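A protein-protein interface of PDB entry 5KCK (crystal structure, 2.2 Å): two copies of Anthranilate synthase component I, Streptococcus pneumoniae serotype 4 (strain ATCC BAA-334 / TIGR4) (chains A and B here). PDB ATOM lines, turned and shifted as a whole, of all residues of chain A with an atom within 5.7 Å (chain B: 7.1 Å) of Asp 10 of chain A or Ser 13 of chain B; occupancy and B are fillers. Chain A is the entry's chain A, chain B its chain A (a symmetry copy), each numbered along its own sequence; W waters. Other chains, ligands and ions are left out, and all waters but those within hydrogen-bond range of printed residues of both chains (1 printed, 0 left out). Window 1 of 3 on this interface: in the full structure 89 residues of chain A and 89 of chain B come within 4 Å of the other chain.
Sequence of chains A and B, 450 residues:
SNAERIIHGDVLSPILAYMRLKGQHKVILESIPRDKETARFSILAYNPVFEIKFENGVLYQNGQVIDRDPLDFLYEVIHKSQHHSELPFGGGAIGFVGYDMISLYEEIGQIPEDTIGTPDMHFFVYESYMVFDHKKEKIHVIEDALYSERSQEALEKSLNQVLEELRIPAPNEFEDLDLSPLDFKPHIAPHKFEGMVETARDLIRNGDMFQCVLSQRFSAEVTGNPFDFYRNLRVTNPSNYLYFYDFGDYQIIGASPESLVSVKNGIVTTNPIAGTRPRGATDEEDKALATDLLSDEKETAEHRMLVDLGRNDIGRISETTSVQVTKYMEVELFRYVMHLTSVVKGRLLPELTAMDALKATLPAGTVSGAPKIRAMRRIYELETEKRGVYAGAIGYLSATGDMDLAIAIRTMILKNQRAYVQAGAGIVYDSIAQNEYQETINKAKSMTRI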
ATOM      1  N   HIS A   8       2.620  -6.837   1.814  1.00  0.00           N
ATOM      2  CA  HIS A   8       1.315  -6.471   1.282  1.00  0.00           C
ATOM      3  C   HIS A   8       0.964  -7.378   0.104  1.00  0.00           C
ATOM      4  O   HIS A   8       1.821  -7.726  -0.716  1.00  0.00           O
ATOM      5  CB  HIS A   8       1.303  -4.999   0.871  1.00  0.00           C
ATOM      6  CG  HIS A   8      -0.013  -4.324   1.106  1.00  0.00           C
ATOM      7  ND1 HIS A   8      -0.776  -3.800   0.083  1.00  0.00           N
ATOM      8  CD2 HIS A   8      -0.707  -4.100   2.247  1.00  0.00           C
ATOM      9  CE1 HIS A   8      -1.882  -3.277   0.584  1.00  0.00           C
ATOM     10  NE2 HIS A   8      -1.867  -3.448   1.894  1.00  0.00           N
ATOM     11  N   GLY A   9      -0.301  -7.791   0.044  1.00  0.00           N
ATOM     12  CA  GLY A   9      -0.720  -8.834  -0.882  1.00  0.00           C
ATOM     13  C   GLY A   9      -0.705  -8.445  -2.353  1.00  0.00           C
ATOM     14  O   GLY A   9      -0.872  -9.327  -3.204  1.00  0.00           O
ATOM     15  N   ASP A  10      -0.499  -7.171  -2.673  1.00  0.00           N
ATOM     16  CA  ASP A  10      -0.657  -6.697  -4.040  1.00  0.00           C
ATOM     17  C   ASP A  10       0.638  -6.705  -4.839  1.00  0.00           C
ATOM     18  O   ASP A  10       0.637  -6.238  -5.983  1.00  0.00           O
ATOM     19  CB  ASP A  10      -1.258  -5.282  -4.048  1.00  0.00           C
ATOM     20  CG  ASP A  10      -0.437  -4.275  -3.231  1.00  0.00           C
ATOM     21  OD1 ASP A  10       0.647  -4.636  -2.727  1.00  0.00           O
ATOM     22  OD2 ASP A  10      -0.872  -3.103  -3.108  1.00  0.00           O
ATOM     23  N   VAL A  11       1.742  -7.196  -4.274  1.00  0.00           N
ATOM     24  CA  VAL A  11       3.024  -7.215  -4.972  1.00  0.00           C
ATOM     25  C   VAL A  11       3.612  -8.610  -5.069  1.00  0.00           C
ATOM     26  O   VAL A  11       4.733  -8.767  -5.567  1.00  0.00           O
ATOM     27  CB  VAL A  11       4.049  -6.256  -4.326  1.00  0.00           C
ATOM     28  CG1 VAL A  11       3.552  -4.839  -4.357  1.00  0.00           C
ATOM     29  CG2 VAL A  11       4.397  -6.704  -2.899  1.00  0.00           C
ATOM     30  N   LEU A  12       2.893  -9.625  -4.611  1.00  0.00           N
ATOM     31  CA  LEU A  12       3.384 -10.990  -4.627  1.00  0.00           C
ATOM     32  C   LEU A  12       2.175 -11.911  -4.641  1.00  0.00           C
ATOM     33  O   LEU A  12       1.212 -11.682  -3.913  1.00  0.00           O
ATOM     34  CB  LEU A  12       4.270 -11.277  -3.404  1.00  0.00           C
ATOM     35  CG  LEU A  12       5.085 -12.572  -3.410  1.00  0.00           C
ATOM     36  CD1 LEU A  12       6.014 -12.600  -4.618  1.00  0.00           C
ATOM     37  CD2 LEU A  12       5.875 -12.701  -2.112  1.00  0.00           C
ATOM     38  N   PHE A 132      -7.647  -6.055 -16.426  1.00  0.00           N
ATOM     39  CA  PHE A 132      -7.519  -7.241 -15.587  1.00  0.00           C
ATOM     40  C   PHE A 132      -8.898  -7.879 -15.471  1.00  0.00           C
ATOM     41  O   PHE A 132      -9.796  -7.315 -14.840  1.00  0.00           O
ATOM     42  CB  PHE A 132      -6.976  -6.885 -14.203  1.00  0.00           C
ATOM     43  CG  PHE A 132      -5.516  -6.506 -14.188  1.00  0.00           C
ATOM     44  CD1 PHE A 132      -5.096  -5.294 -14.706  1.00  0.00           C
ATOM     45  CD2 PHE A 132      -4.569  -7.354 -13.619  1.00  0.00           C
ATOM     46  CE1 PHE A 132      -3.749  -4.937 -14.684  1.00  0.00           C
ATOM     47  CE2 PHE A 132      -3.226  -7.005 -13.592  1.00  0.00           C
ATOM     48  CZ  PHE A 132      -2.816  -5.796 -14.128  1.00  0.00           C
ATOM     49  N   ILE A 139      -5.150 -11.192 -18.171  1.00  0.00           N
ATOM     50  CA  ILE A 139      -4.804  -9.789 -18.309  1.00  0.00           C
ATOM     51  C   ILE A 139      -4.698  -9.471 -19.795  1.00  0.00           C
ATOM     52  O   ILE A 139      -3.911 -10.096 -20.512  1.00  0.00           O
ATOM     53  CB  ILE A 139      -3.500  -9.463 -17.577  1.00  0.00           C
ATOM     54  CG1 ILE A 139      -3.578  -9.929 -16.114  1.00  0.00           C
ATOM     55  CG2 ILE A 139      -3.255  -8.008 -17.647  1.00  0.00           C
ATOM     56  CD1 ILE A 139      -2.284  -9.730 -15.358  1.00  0.00           C
ATOM     57  N   ARG A 231      -3.055   1.982  -2.418  1.00  0.00           N
ATOM     58  CA  ARG A 231      -2.853   0.554  -2.184  1.00  0.00           C
ATOM     59  C   ARG A 231      -3.534   0.109  -0.898  1.00  0.00           C
ATOM     60  O   ARG A 231      -4.105  -0.987  -0.832  1.00  0.00           O
ATOM     61  CB  ARG A 231      -1.358   0.221  -2.134  1.00  0.00           C
ATOM     62  CG  ARG A 231      -0.614   0.449  -3.450  1.00  0.00           C
ATOM     63  CD  ARG A 231       0.897   0.278  -3.242  1.00  0.00           C
ATOM     64  NE  ARG A 231       1.208  -1.063  -2.756  1.00  0.00           N
ATOM     65  CZ  ARG A 231       2.385  -1.433  -2.262  1.00  0.00           C
ATOM     66  NH1 ARG A 231       3.385  -0.561  -2.170  1.00  0.00           N
ATOM     67  NH2 ARG A 231       2.553  -2.678  -1.848  1.00  0.00           N
ATOM     68  N   ARG A 234      -7.660   0.292  -1.343  1.00  0.00           N
ATOM     69  CA  ARG A 234      -8.350  -0.768  -2.065  1.00  0.00           C
ATOM     70  C   ARG A 234      -8.440  -2.052  -1.254  1.00  0.00           C
ATOM     71  O   ARG A 234      -9.260  -2.915  -1.581  1.00  0.00           O
ATOM     72  CB  ARG A 234      -7.677  -1.018  -3.424  1.00  0.00           C
ATOM     73  CG  ARG A 234      -6.223  -1.413  -3.356  1.00  0.00           C
ATOM     74  CD  ARG A 234      -5.490  -1.131  -4.679  1.00  0.00           C
ATOM     75  NE  ARG A 234      -5.898  -1.987  -5.795  1.00  0.00           N
ATOM     76  CZ  ARG A 234      -5.653  -3.295  -5.871  1.00  0.00           C
ATOM     77  NH1 ARG A 234      -5.012  -3.927  -4.888  1.00  0.00           N
ATOM     78  NH2 ARG A 234      -6.059  -3.979  -6.930  1.00  0.00           N
ATOM     79  N   HIS B   8      -1.099 -14.238 -18.061  1.00  0.00           N
ATOM     80  CA  HIS B   8      -1.757 -15.005 -17.013  1.00  0.00           C
ATOM     81  C   HIS B   8      -1.813 -14.182 -15.728  1.00  0.00           C
ATOM     82  O   HIS B   8      -0.867 -13.465 -15.383  1.00  0.00           O
ATOM     83  CB  HIS B   8      -1.031 -16.331 -16.789  1.00  0.00           C
ATOM     84  CG  HIS B   8      -1.947 -17.462 -16.437  1.00  0.00           C
ATOM     85  ND1 HIS B   8      -1.881 -18.128 -15.231  1.00  0.00           N
ATOM     86  CD2 HIS B   8      -2.961 -18.034 -17.128  1.00  0.00           C
ATOM     87  CE1 HIS B   8      -2.811 -19.067 -15.196  1.00  0.00           C
ATOM     88  NE2 HIS B   8      -3.483 -19.030 -16.333  1.00  0.00           N
ATOM     89  N   GLY B   9      -2.949 -14.258 -15.036  1.00  0.00           N
ATOM     90  CA  GLY B   9      -3.229 -13.358 -13.926  1.00  0.00           C
ATOM     91  C   GLY B   9      -2.377 -13.570 -12.683  1.00  0.00           C
ATOM     92  O   GLY B   9      -2.432 -12.733 -11.773  1.00  0.00           O
ATOM     93  N   ASP B  10      -1.592 -14.642 -12.624  1.00  0.00           N
ATOM     94  CA  ASP B  10      -0.897 -15.006 -11.398  1.00  0.00           C
ATOM     95  C   ASP B  10       0.515 -14.445 -11.311  1.00  0.00           C
ATOM     96  O   ASP B  10       1.228 -14.768 -10.355  1.00  0.00           O
ATOM     97  CB  ASP B  10      -0.854 -16.535 -11.243  1.00  0.00           C
ATOM     98  CG  ASP B  10      -0.214 -17.244 -12.445  1.00  0.00           C
ATOM     99  OD1 ASP B  10       0.282 -16.560 -13.364  1.00  0.00           O
ATOM    100  OD2 ASP B  10      -0.190 -18.500 -12.459  1.00  0.00           O
ATOM    101  N   VAL B  11       0.950 -13.640 -12.281  1.00  0.00           N
ATOM    102  CA  VAL B  11       2.300 -13.085 -12.276  1.00  0.00           C
ATOM    103  C   VAL B  11       2.304 -11.569 -12.335  1.00  0.00           C
ATOM    104  O   VAL B  11       3.379 -10.963 -12.415  1.00  0.00           O
ATOM    105  CB  VAL B  11       3.167 -13.657 -13.420  1.00  0.00           C
ATOM    106  CG1 VAL B  11       3.304 -15.147 -13.294  1.00  0.00           C
ATOM    107  CG2 VAL B  11       2.605 -13.253 -14.790  1.00  0.00           C
ATOM    108  N   LEU B  12       1.139 -10.938 -12.296  1.00  0.00           N
ATOM    109  CA  LEU B  12       1.037  -9.493 -12.383  1.00  0.00           C
ATOM    110  C   LEU B  12      -0.262  -9.084 -11.710  1.00  0.00           C
ATOM    111  O   LEU B  12      -1.294  -9.720 -11.913  1.00  0.00           O
ATOM    112  CB  LEU B  12       1.062  -9.020 -13.846  1.00  0.00           C
ATOM    113  CG  LEU B  12       1.241  -7.523 -14.102  1.00  0.00           C
ATOM    114  CD1 LEU B  12       2.547  -7.039 -13.482  1.00  0.00           C
ATOM    115  CD2 LEU B  12       1.211  -7.239 -15.600  1.00  0.00           C
ATOM    116  N   SER B  13      -0.194  -8.045 -10.894  1.00  0.00           N
ATOM    117  CA  SER B  13      -1.343  -7.388 -10.308  1.00  0.00           C
ATOM    118  C   SER B  13      -1.465  -5.977 -10.880  1.00  0.00           C
ATOM    119  O   SER B  13      -0.523  -5.470 -11.500  1.00  0.00           O
ATOM    120  CB  SER B  13      -1.199  -7.327  -8.782  1.00  0.00           C
ATOM    121  OG  SER B  13      -0.256  -6.328  -8.442  1.00  0.00           O
ATOM    122  N   PRO B  14      -2.617  -5.315 -10.719  1.00  0.00           N
ATOM    123  CA  PRO B  14      -2.717  -3.938 -11.235  1.00  0.00           C
ATOM    124  C   PRO B  14      -1.810  -2.969 -10.497  1.00  0.00           C
ATOM    125  O   PRO B  14      -1.366  -1.975 -11.086  1.00  0.00           O
ATOM    126  CB  PRO B  14      -4.206  -3.586 -11.065  1.00  0.00           C
ATOM    127  CG  PRO B  14      -4.750  -4.563 -10.125  1.00  0.00           C
ATOM    128  CD  PRO B  14      -3.901  -5.809 -10.195  1.00  0.00           C
ATOM    129  N   ILE B  15      -1.492  -3.244  -9.235  1.00  0.00           N
ATOM    130  CA  ILE B  15      -0.521  -2.419  -8.529  1.00  0.00           C
ATOM    131  C   ILE B  15       0.869  -2.594  -9.130  1.00  0.00           C
ATOM    132  O   ILE B  15       1.560  -1.611  -9.430  1.00  0.00           O
ATOM    133  CB  ILE B  15      -0.536  -2.743  -7.027  1.00  0.00           C
ATOM    134  CG1 ILE B  15      -1.919  -2.417  -6.448  1.00  0.00           C
ATOM    135  CG2 ILE B  15       0.587  -1.992  -6.310  1.00  0.00           C
ATOM    136  CD1 ILE B  15      -2.392  -0.998  -6.724  1.00  0.00           C
ATOM    137  N   LEU B  16       1.301  -3.849  -9.315  1.00  0.00           N
ATOM    138  CA  LEU B  16       2.606  -4.095  -9.925  1.00  0.00           C
ATOM    139  C   LEU B  16       2.691  -3.473 -11.312  1.00  0.00           C
ATOM    140  O   LEU B  16       3.716  -2.889 -11.677  1.00  0.00           O
ATOM    141  CB  LEU B  16       2.891  -5.593 -10.007  1.00  0.00           C
ATOM    142  CG  LEU B  16       3.248  -6.356  -8.727  1.00  0.00           C
ATOM    143  CD1 LEU B  16       3.485  -7.821  -9.053  1.00  0.00           C
ATOM    144  CD2 LEU B  16       4.481  -5.756  -8.050  1.00  0.00           C
ATOM    145  N   ALA B  17       1.626  -3.589 -12.104  1.00  0.00           N
ATOM    146  CA  ALA B  17       1.650  -2.981 -13.429  1.00  0.00           C
ATOM    147  C   ALA B  17       1.842  -1.475 -13.329  1.00  0.00           C
ATOM    148  O   ALA B  17       2.681  -0.893 -14.030  1.00  0.00           O
ATOM    149  CB  ALA B  17       0.369  -3.321 -14.195  1.00  0.00           C
ATOM    150  N   TYR B  18       1.087  -0.825 -12.438  1.00  0.00           N
ATOM    151  CA  TYR B  18       1.189   0.627 -12.305  1.00  0.00           C
ATOM    152  C   TYR B  18       2.608   1.053 -11.944  1.00  0.00           C
ATOM    153  O   TYR B  18       3.156   1.995 -12.531  1.00  0.00           O
ATOM    154  CB  TYR B  18       0.203   1.127 -11.255  1.00  0.00           C
ATOM    155  CG  TYR B  18      -0.029   2.618 -11.315  1.00  0.00           C
ATOM    156  CD1 TYR B  18       0.818   3.514 -10.663  1.00  0.00           C
ATOM    157  CD2 TYR B  18      -1.086   3.129 -12.036  1.00  0.00           C
ATOM    158  CE1 TYR B  18       0.590   4.883 -10.726  1.00  0.00           C
ATOM    159  CE2 TYR B  18      -1.331   4.482 -12.093  1.00  0.00           C
ATOM    160  CZ  TYR B  18      -0.488   5.355 -11.448  1.00  0.00           C
ATOM    161  OH  TYR B  18      -0.753   6.698 -11.541  1.00  0.00           O
ATOM    162  N   MET B  19       3.220   0.366 -10.983  1.00  0.00           N
ATOM    163  CA  MET B  19       4.555   0.726 -10.526  1.00  0.00           C
ATOM    164  C   MET B  19       5.619   0.536 -11.606  1.00  0.00           C
ATOM    165  O   MET B  19       6.612   1.259 -11.634  1.00  0.00           O
ATOM    166  CB  MET B  19       4.932  -0.093  -9.292  1.00  0.00           C
ATOM    167  CG  MET B  19       4.121   0.223  -8.050  1.00  0.00           C
ATOM    168  SD  MET B  19       4.505  -1.035  -6.568  1.00  0.00           S
ATOM    169  CE  MET B  19       4.265   0.221  -5.095  1.00  0.00           C
ATOM    170  N   ARG B  20       5.416  -0.450 -12.485  1.00  0.00           N
ATOM    171  CA  ARG B  20       6.415  -0.787 -13.495  1.00  0.00           C
ATOM    172  C   ARG B  20       6.222  -0.031 -14.804  1.00  0.00           C
ATOM    173  O   ARG B  20       7.202   0.192 -15.525  1.00  0.00           O
ATOM    174  CB  ARG B  20       6.399  -2.295 -13.777  1.00  0.00           C
ATOM    175  CG  ARG B  20       6.802  -3.166 -12.581  1.00  0.00           C
ATOM    176  CD  ARG B  20       6.677  -4.651 -12.897  1.00  0.00           C
ATOM    177  NE  ARG B  20       6.911  -5.481 -11.719  1.00  0.00           N
ATOM    178  CZ  ARG B  20       6.790  -6.809 -11.694  1.00  0.00           C
ATOM    179  NH1 ARG B  20       6.432  -7.463 -12.790  1.00  0.00           N
ATOM    180  NH2 ARG B  20       7.025  -7.483 -10.568  1.00  0.00           N
ATOM    181  N   GLU B 137      -5.455  -9.800   2.365  1.00  0.00           N
ATOM    182  CA  GLU B 137      -4.420  -9.374   1.416  1.00  0.00           C
ATOM    183  C   GLU B 137      -3.100  -9.114   2.131  1.00  0.00           C
ATOM    184  O   GLU B 137      -2.412  -8.126   1.872  1.00  0.00           O
ATOM    185  CB  GLU B 137      -4.857  -8.138   0.628  1.00  0.00           C
ATOM    186  CG  GLU B 137      -5.887  -8.418  -0.455  1.00  0.00           C
ATOM    187  CD  GLU B 137      -5.362  -9.376  -1.517  1.00  0.00           C
ATOM    188  OE1 GLU B 137      -4.179  -9.247  -1.905  1.00  0.00           O
ATOM    189  OE2 GLU B 137      -6.126 -10.265  -1.953  1.00  0.00           O
ATOM    190  N   LYS B 138      -2.763  -9.997   3.065  1.00  0.00           N
ATOM    191  CA  LYS B 138      -1.517  -9.922   3.809  1.00  0.00           C
ATOM    192  C   LYS B 138      -0.768 -11.232   3.637  1.00  0.00           C
ATOM    193  O   LYS B 138      -1.372 -12.310   3.588  1.00  0.00           O
ATOM    194  CB  LYS B 138      -1.750  -9.636   5.300  1.00  0.00           C
ATOM    195  CG  LYS B 138      -2.219  -8.207   5.614  1.00  0.00           C
ATOM    196  CD  LYS B 138      -1.205  -7.163   5.152  1.00  0.00           C
ATOM    197  CE  LYS B 138      -1.602  -5.744   5.565  1.00  0.00           C
ATOM    198  NZ  LYS B 138      -2.763  -5.236   4.789  1.00  0.00           N
ATOM    199  N   ILE B 139       0.550 -11.133   3.534  1.00  0.00           N
ATOM    200  CA  ILE B 139       1.407 -12.291   3.355  1.00  0.00           C
ATOM    201  C   ILE B 139       2.313 -12.402   4.575  1.00  0.00           C
ATOM    202  O   ILE B 139       3.053 -11.465   4.891  1.00  0.00           O
ATOM    203  CB  ILE B 139       2.224 -12.183   2.066  1.00  0.00           C
ATOM    204  CG1 ILE B 139       1.297 -11.923   0.867  1.00  0.00           C
ATOM    205  CG2 ILE B 139       2.988 -13.433   1.870  1.00  0.00           C
ATOM    206  CD1 ILE B 139       2.048 -11.704  -0.427  1.00  0.00           C
HETATM  207  O   HOH W   1       7.028  -8.653  -7.343  1.00  0.00           O
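Glu 137 of chain B touches His 8 of chain A.
NZ of Lys 138 of chain B touches CD2 of His 8 of chain A (3.5 Å).
Ile 15 of chain B touches Asp 10 of chain A (CG1 to OD2, 3.6 Å).
CA of Val 11 of chain A touches CD2 of Leu 16 of chain B, 3.7 Å away.
Ile 139 of chain B touches Leu 12 of chain A.
Phe 132 of chain A touches Leu 12 of chain B.
Leu 12 of chain B touches Ile 139 of chain A (O to CD1, 3.6 Å).
Arg 231 of chain A touches Met 19 of chain B.
NH2 of Arg 234 of chain A touches CG of Pro 14 of chain B, 3.5 Å away.
Ile 15 of chain B touches Arg 234 of chain A (CD1 to CD, 3.7 Å).
A ring nitrogen (ND1) of His 8 of chain A lies within hydrogen-bond range of the side-chain carboxylate (OD1) of Asp 10 of chain A, 3.3 Å away.
NH2 of Arg 231 of chain A is in salt-bridge range of OD1 of Asp 10 of chain A, 2.9 Å away.
ND1 of His 8 of chain B lies within hydrogen-bond range of OD1 of Asp 10 of chain B (3.3 Å).
OG of Ser 13 of chain B sits close to N of Ile 15 of chain B (3.4 Å).
The backbone NH (N) of Leu 16 of chain B lies within hydrogen-bond range of the side-chain hydroxyl (OG) of Ser 13 of chain B, at 3.1 Å.
Of the 9 printed residues of chain A, 9 touch a printed residue of chain B.
Among the printed residues, no Asp or Glu carboxylate lies within 4 Å of a Lys or Arg side-chain nitrogen of the other chain.
Asp 10 of chain A touches three residues of chain B.
Ser 13 of chain B touches just these residues of chain A: Asp 10 and Phe 132.
Of the printed residues of chain A, Glu 137 of chain B touches His 8 and Gly 9.
Printed residues of chain A within 4 Å of Met 19 of chain B: Arg 231 (3.2 Å).
Of the printed residues of chain B, Phe 132 of chain A touches Leu 12 (3.7 Å), Ser 13 (3.4 Å) and Pro 14 (3.4 Å).
Of the printed residues of chain B, Gly 9 of chain A touches Glu 137 (2.8 Å).
Of the printed residues of chain B, Ile 139 of chain A touches His 8 and Leu 12.
Ala 17 of chain B touches none of the printed residues of chain A.
Val 11 of chain B touches none of the printed residues of chain A.
The nearest residue of chain B that does not touch Asp 10 of chain A is Glu 137 of chain B (4.3 Å).
The nearest printed residue of chain A that does not touch His 8 of chain B is Phe 132 of chain A (7.1 Å).
Water W1 bridges the backbone carbonyl oxygen (O) of Val 11 of chain A (2.9 Å) and the guanidinium group (NH2) of Arg 20 of chain B (3.4 Å).
The backbone NH (N) of Gly 9 of chain A sits at hydrogen-bond distance from the backbone carbonyl oxygen (O) of Glu 137 of chain B (2.8 Å).
The side-chain hydroxyl (OG) of Ser 13 of chain B lies within hydrogen-bond range of the backbone carbonyl oxygen (O) of Asp 10 of chain A.
His 8 of chain A touches Ile 139 of chain B, and with the chains exchanged Ile 139 of chain A touches His 8 of chain B.
Leu 12 of chain A touches Ile 139 of chain B, and with the chains exchanged Ile 139 of chain A touches Leu 12 of chain B.
Positions printed for both chains: 8, 9, 10, 11, 12 and 139.
Of the 18 pairs that touch across the chains among the printed residues, 4 have their exchanged pair printed and touching as well.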
